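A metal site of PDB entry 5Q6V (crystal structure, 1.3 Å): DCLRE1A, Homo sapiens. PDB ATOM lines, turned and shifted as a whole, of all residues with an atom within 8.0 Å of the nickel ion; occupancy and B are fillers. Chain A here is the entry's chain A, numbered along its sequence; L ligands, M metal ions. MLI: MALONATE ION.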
ATOM      1  N   ASP A  18      16.072 -34.396 -25.511  1.00  0.00           N
ATOM      2  CA  ASP A  18      14.849 -33.948 -26.252  1.00  0.00           C
ATOM      3  C   ASP A  18      14.613 -34.758 -27.595  1.00  0.00           C
ATOM      4  O   ASP A  18      14.242 -34.163 -28.639  1.00  0.00           O
ATOM      5  CB  ASP A  18      14.779 -32.472 -26.433  1.00  0.00           C
ATOM      6  CG  ASP A  18      14.887 -31.688 -25.072  1.00  0.00           C
ATOM      7  OD1 ASP A  18      14.658 -32.355 -24.022  1.00  0.00           O
ATOM      8  OD2 ASP A  18      15.092 -30.438 -25.181  1.00  0.00           O
ATOM      9  N   THR A  34      14.588 -31.684 -21.255  1.00  0.00           N
ATOM     10  CA  THR A  34      14.939 -30.377 -20.666  1.00  0.00           C
ATOM     11  C   THR A  34      13.712 -29.667 -20.055  1.00  0.00           C
ATOM     12  O   THR A  34      13.856 -28.976 -19.042  1.00  0.00           O
ATOM     13  CB  THR A  34      15.682 -29.455 -21.627  1.00  0.00           C
ATOM     14  OG1 THR A  34      14.838 -29.113 -22.754  1.00  0.00           O
ATOM     15  CG2 THR A  34      17.001 -30.075 -22.139  1.00  0.00           C
ATOM     16  N   HIS A  35      12.529 -29.817 -20.726  1.00  0.00           N
ATOM     17  CA  HIS A  35      11.324 -29.071 -20.299  1.00  0.00           C
ATOM     18  C   HIS A  35      10.107 -29.627 -20.986  1.00  0.00           C
ATOM     19  O   HIS A  35      10.206 -30.245 -22.084  1.00  0.00           O
ATOM     20  CB  HIS A  35      11.476 -27.515 -20.512  1.00  0.00           C
ATOM     21  CG  HIS A  35      11.543 -27.035 -21.917  1.00  0.00           C
ATOM     22  ND1 HIS A  35      12.572 -27.276 -22.793  1.00  0.00           N
ATOM     23  CD2 HIS A  35      10.639 -26.277 -22.611  1.00  0.00           C
ATOM     24  CE1 HIS A  35      12.314 -26.651 -23.941  1.00  0.00           C
ATOM     25  NE2 HIS A  35      11.165 -26.027 -23.814  1.00  0.00           N
ATOM     26  N   PHE A  36       8.964 -29.348 -20.387  1.00  0.00           N
ATOM     27  CA  PHE A  36       7.658 -29.802 -20.949  1.00  0.00           C
ATOM     28  C   PHE A  36       7.046 -28.845 -21.981  1.00  0.00           C
ATOM     29  O   PHE A  36       5.933 -28.250 -21.696  1.00  0.00           O
ATOM     30  CB  PHE A  36       6.707 -30.071 -19.765  1.00  0.00           C
ATOM     31  CG  PHE A  36       5.498 -30.947 -20.060  1.00  0.00           C
ATOM     32  CD1 PHE A  36       5.639 -32.303 -20.184  1.00  0.00           C
ATOM     33  CD2 PHE A  36       4.218 -30.343 -20.226  1.00  0.00           C
ATOM     34  CE1 PHE A  36       4.515 -33.087 -20.516  1.00  0.00           C
ATOM     35  CE2 PHE A  36       3.072 -31.119 -20.482  1.00  0.00           C
ATOM     36  CZ  PHE A  36       3.242 -32.484 -20.627  1.00  0.00           C
ATOM     37  N   HIS A  37       7.655 -28.744 -23.174  1.00  0.00           N
ATOM     38  CA  HIS A  37       7.104 -28.074 -24.365  1.00  0.00           C
ATOM     39  C   HIS A  37       7.010 -29.144 -25.463  1.00  0.00           C
ATOM     40  O   HIS A  37       7.904 -29.990 -25.605  1.00  0.00           O
ATOM     41  CB  HIS A  37       7.881 -26.849 -24.834  1.00  0.00           C
ATOM     42  CG  HIS A  37       7.595 -25.590 -24.071  1.00  0.00           C
ATOM     43  ND1 HIS A  37       8.420 -24.492 -24.110  1.00  0.00           N
ATOM     44  CD2 HIS A  37       6.564 -25.254 -23.264  1.00  0.00           C
ATOM     45  CE1 HIS A  37       7.899 -23.526 -23.367  1.00  0.00           C
ATOM     46  NE2 HIS A  37       6.799 -23.975 -22.822  1.00  0.00           N
ATOM     47  N   SER A  38       5.931 -29.110 -26.271  1.00  0.00           N
ATOM     48  CA  SER A  38       5.574 -30.227 -27.170  1.00  0.00           C
ATOM     49  C   SER A  38       6.635 -30.492 -28.201  1.00  0.00           C
ATOM     50  O   SER A  38       6.851 -31.694 -28.472  1.00  0.00           O
ATOM     51  CB  SER A  38       4.132 -30.044 -27.696  1.00  0.00           C
ATOM     52  OG  SER A  38       4.081 -28.893 -28.510  1.00  0.00           O
ATOM     53  N   ASP A  39       7.322 -29.490 -28.731  1.00  0.00           N
ATOM     54  CA  ASP A  39       8.394 -29.772 -29.759  1.00  0.00           C
ATOM     55  C   ASP A  39       9.506 -30.591 -29.131  1.00  0.00           C
ATOM     56  O   ASP A  39      10.318 -31.253 -29.836  1.00  0.00           O
ATOM     57  CB  ASP A  39       8.945 -28.506 -30.332  1.00  0.00           C
ATOM     58  CG  ASP A  39       8.069 -27.902 -31.544  1.00  0.00           C
ATOM     59  OD1 ASP A  39       7.043 -28.529 -31.918  1.00  0.00           O
ATOM     60  OD2 ASP A  39       8.446 -26.815 -31.987  1.00  0.00           O
ATOM     61  N   HIS A  40       9.621 -30.552 -27.791  1.00  0.00           N
ATOM     62  CA  HIS A  40      10.665 -31.310 -27.099  1.00  0.00           C
ATOM     63  C   HIS A  40      10.239 -32.630 -26.513  1.00  0.00           C
ATOM     64  O   HIS A  40      11.059 -33.594 -26.603  1.00  0.00           O
ATOM     65  CB  HIS A  40      11.270 -30.367 -25.963  1.00  0.00           C
ATOM     66  CG  HIS A  40      11.871 -29.114 -26.506  1.00  0.00           C
ATOM     67  ND1 HIS A  40      13.223 -28.885 -26.638  1.00  0.00           N
ATOM     68  CD2 HIS A  40      11.276 -27.999 -27.006  1.00  0.00           C
ATOM     69  CE1 HIS A  40      13.434 -27.740 -27.239  1.00  0.00           C
ATOM     70  NE2 HIS A  40      12.249 -27.183 -27.474  1.00  0.00           N
ATOM     71  N   HIS A  96      13.482 -20.401 -18.234  1.00  0.00           N
ATOM     72  CA  HIS A  96      12.565 -20.586 -19.396  1.00  0.00           C
ATOM     73  C   HIS A  96      11.186 -20.702 -18.801  1.00  0.00           C
ATOM     74  O   HIS A  96      10.741 -19.671 -18.172  1.00  0.00           O
ATOM     75  CB  HIS A  96      13.017 -21.744 -20.326  1.00  0.00           C
ATOM     76  CG  HIS A  96      12.238 -21.990 -21.604  1.00  0.00           C
ATOM     77  ND1 HIS A  96      11.990 -20.978 -22.500  1.00  0.00           N
ATOM     78  CD2 HIS A  96      11.661 -23.112 -22.075  1.00  0.00           C
ATOM     79  CE1 HIS A  96      11.315 -21.514 -23.518  1.00  0.00           C
ATOM     80  NE2 HIS A  96      11.113 -22.797 -23.306  1.00  0.00           N
ATOM     81  N   CYS A  97      10.503 -21.818 -18.919  1.00  0.00           N
ATOM     82  CA  CYS A  97       9.177 -22.118 -18.265  1.00  0.00           C
ATOM     83  C   CYS A  97       9.396 -22.913 -16.989  1.00  0.00           C
ATOM     84  O   CYS A  97      10.512 -23.379 -16.725  1.00  0.00           O
ATOM     85  CB  CYS A  97       8.293 -22.847 -19.282  1.00  0.00           C
ATOM     86  SG  CYS A  97       8.950 -24.548 -19.726  1.00  0.00           S
ATOM     87  N   ALA A 100      12.053 -26.038 -16.403  1.00  0.00           N
ATOM     88  CA  ALA A 100      13.033 -26.113 -17.493  1.00  0.00           C
ATOM     89  C   ALA A 100      14.462 -26.031 -16.935  1.00  0.00           C
ATOM     90  O   ALA A 100      14.762 -25.172 -16.052  1.00  0.00           O
ATOM     91  CB  ALA A 100      12.802 -24.997 -18.481  1.00  0.00           C
ATOM     92  N   GLY A 117      19.225 -26.495 -23.259  1.00  0.00           N
ATOM     93  CA  GLY A 117      17.812 -26.667 -23.594  1.00  0.00           C
ATOM     94  C   GLY A 117      17.304 -25.400 -24.222  1.00  0.00           C
ATOM     95  O   GLY A 117      18.034 -24.712 -24.941  1.00  0.00           O
ATOM     96  N   ASP A 118      16.058 -25.027 -23.879  1.00  0.00           N
ATOM     97  CA  ASP A 118      15.572 -23.643 -24.147  1.00  0.00           C
ATOM     98  C   ASP A 118      15.905 -22.742 -22.903  1.00  0.00           C
ATOM     99  O   ASP A 118      15.673 -23.192 -21.784  1.00  0.00           O
ATOM    100  CB  ASP A 118      14.078 -23.598 -24.414  1.00  0.00           C
ATOM    101  CG  ASP A 118      13.647 -24.052 -25.820  1.00  0.00           C
ATOM    102  OD1 ASP A 118      14.517 -24.180 -26.716  1.00  0.00           O
ATOM    103  OD2 ASP A 118      12.405 -24.132 -26.032  1.00  0.00           O
ATOM    104  N   PHE A 119      16.454 -21.546 -23.103  1.00  0.00           N
ATOM    105  CA  PHE A 119      16.812 -20.679 -21.972  1.00  0.00           C
ATOM    106  C   PHE A 119      16.700 -19.187 -22.290  1.00  0.00           C
ATOM    107  O   PHE A 119      16.721 -18.786 -23.462  1.00  0.00           O
ATOM    108  CB  PHE A 119      18.257 -21.042 -21.403  1.00  0.00           C
ATOM    109  CG  PHE A 119      19.489 -20.400 -22.053  1.00  0.00           C
ATOM    110  CD1 PHE A 119      20.541 -19.964 -21.273  1.00  0.00           C
ATOM    111  CD2 PHE A 119      19.608 -20.285 -23.447  1.00  0.00           C
ATOM    112  CE1 PHE A 119      21.714 -19.464 -21.845  1.00  0.00           C
ATOM    113  CE2 PHE A 119      20.762 -19.726 -24.021  1.00  0.00           C
ATOM    114  CZ  PHE A 119      21.806 -19.334 -23.187  1.00  0.00           C
ATOM    115  N   ASP A 141      20.678 -22.727 -27.341  1.00  0.00           N
ATOM    116  CA  ASP A 141      19.343 -22.245 -27.840  1.00  0.00           C
ATOM    117  C   ASP A 141      19.589 -20.918 -28.547  1.00  0.00           C
ATOM    118  O   ASP A 141      19.784 -19.850 -27.929  1.00  0.00           O
ATOM    119  CB  ASP A 141      18.409 -22.036 -26.648  1.00  0.00           C
ATOM    120  CG  ASP A 141      17.129 -21.268 -26.990  1.00  0.00           C
ATOM    121  OD1 ASP A 141      16.867 -21.098 -28.208  1.00  0.00           O
ATOM    122  OD2 ASP A 141      16.444 -20.839 -26.044  1.00  0.00           O
ATOM    123  N   THR A 143      17.400 -19.411 -30.725  1.00  0.00           N
ATOM    124  CA  THR A 143      16.115 -18.935 -31.232  1.00  0.00           C
ATOM    125  C   THR A 143      16.212 -17.534 -31.766  1.00  0.00           C
ATOM    126  O   THR A 143      15.823 -17.286 -32.981  1.00  0.00           O
ATOM    127  CB  THR A 143      15.024 -19.042 -30.141  1.00  0.00           C
ATOM    128  OG1 THR A 143      14.808 -20.395 -29.782  1.00  0.00           O
ATOM    129  CG2 THR A 143      13.691 -18.504 -30.674  1.00  0.00           C
ATOM    130  N   SER A 183       0.601 -23.309 -23.726  1.00  0.00           N
ATOM    131  CA  SER A 183       1.640 -24.171 -23.189  1.00  0.00           C
ATOM    132  C   SER A 183       1.956 -23.644 -21.785  1.00  0.00           C
ATOM    133  O   SER A 183       1.553 -22.494 -21.425  1.00  0.00           O
ATOM    134  CB  SER A 183       2.960 -24.032 -23.986  1.00  0.00           C
ATOM    135  OG  SER A 183       3.414 -22.696 -24.015  1.00  0.00           O
ATOM    136  N   ILE A 184       2.727 -24.351 -20.995  1.00  0.00           N
ATOM    137  CA  ILE A 184       3.237 -23.791 -19.767  1.00  0.00           C
ATOM    138  C   ILE A 184       4.262 -22.705 -20.094  1.00  0.00           C
ATOM    139  O   ILE A 184       4.806 -22.624 -21.242  1.00  0.00           O
ATOM    140  CB  ILE A 184       3.889 -24.851 -18.818  1.00  0.00           C
ATOM    141  CG1 ILE A 184       5.146 -25.495 -19.409  1.00  0.00           C
ATOM    142  CG2 ILE A 184       2.861 -25.876 -18.363  1.00  0.00           C
ATOM    143  CD1 ILE A 184       5.942 -26.300 -18.409  1.00  0.00           C
ATOM    144  N   GLU A 296      10.507 -15.787 -23.087  1.00  0.00           N
ATOM    145  CA  GLU A 296      11.259 -16.779 -22.251  1.00  0.00           C
ATOM    146  C   GLU A 296      12.486 -17.374 -22.975  1.00  0.00           C
ATOM    147  O   GLU A 296      13.020 -18.412 -22.593  1.00  0.00           O
ATOM    148  CB  GLU A 296      10.327 -17.835 -21.665  1.00  0.00           C
ATOM    149  CG  GLU A 296       9.360 -17.237 -20.559  1.00  0.00           C
ATOM    150  CD  GLU A 296       8.482 -18.230 -19.812  1.00  0.00           C
ATOM    151  OE1 GLU A 296       8.253 -19.374 -20.319  1.00  0.00           O
ATOM    152  OE2 GLU A 296       7.969 -17.877 -18.692  1.00  0.00           O
ATOM    153  N   HIS A 297      12.920 -16.660 -24.049  1.00  0.00           N
ATOM    154  CA  HIS A 297      14.206 -16.932 -24.700  1.00  0.00           C
ATOM    155  C   HIS A 297      15.124 -15.710 -24.653  1.00  0.00           C
ATOM    156  O   HIS A 297      14.683 -14.530 -24.622  1.00  0.00           O
ATOM    157  CB  HIS A 297      13.999 -17.317 -26.226  1.00  0.00           C
ATOM    158  CG  HIS A 297      13.266 -18.572 -26.478  1.00  0.00           C
ATOM    159  ND1 HIS A 297      13.854 -19.818 -26.512  1.00  0.00           N
ATOM    160  CD2 HIS A 297      11.938 -18.803 -26.746  1.00  0.00           C
ATOM    161  CE1 HIS A 297      12.946 -20.730 -26.829  1.00  0.00           C
ATOM    162  NE2 HIS A 297      11.781 -20.134 -26.937  1.00  0.00           N
HETATM  163  C1  MLI L   1       8.486 -23.440 -27.535  1.00  0.00           C
HETATM  164  C2  MLI L   1       9.317 -22.241 -27.087  1.00  0.00           C
HETATM  165  C3  MLI L   1       9.281 -24.737 -27.650  1.00  0.00           C
HETATM  166  O6  MLI L   1       9.389 -21.169 -27.704  1.00  0.00           O
HETATM  167  O7  MLI L   1       9.885 -22.420 -26.065  1.00  0.00           O
HETATM  168  O8  MLI L   1       9.911 -25.181 -26.704  1.00  0.00           O
HETATM  169  O9  MLI L   1       9.160 -25.453 -28.686  1.00  0.00           O
HETATM  170 NI    NI M   1      10.490 -24.216 -24.991  1.00  0.00          NI
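A ring nitrogen (NE2) of His 40 sits close to the side-chain carboxylate of Asp 118 (3.4 Å).
A ring nitrogen (ND1) of His 35 sits at hydrogen-bond distance from the side-chain hydroxyl (OG1) of Thr 34 (2.9 Å).
O of Ile 184 sits at hydrogen-bond distance from NE2 of His 37, 2.9 Å away.
O of Glu 296 sits at hydrogen-bond distance from ND1 of His 96 (2.8 Å).
Within 4 Å of the nickel ion: His 35, His 37, His 96 and Asp 118.
The nickel ion is bound by an oxygen (O8) of the ligand (2.0 Å), an oxygen (O7) of the ligand (2.2 Å), the side-chain carboxylate (OD2) of Asp 118 (2.2 Å), a ring nitrogen (NE2) of His 35 (2.3 Å), a ring nitrogen (ND1) of His 37 (2.3 Å) and a ring nitrogen (NE2) of His 96 (2.3 Å).
The nickel ion has six donor atoms within binding distance.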
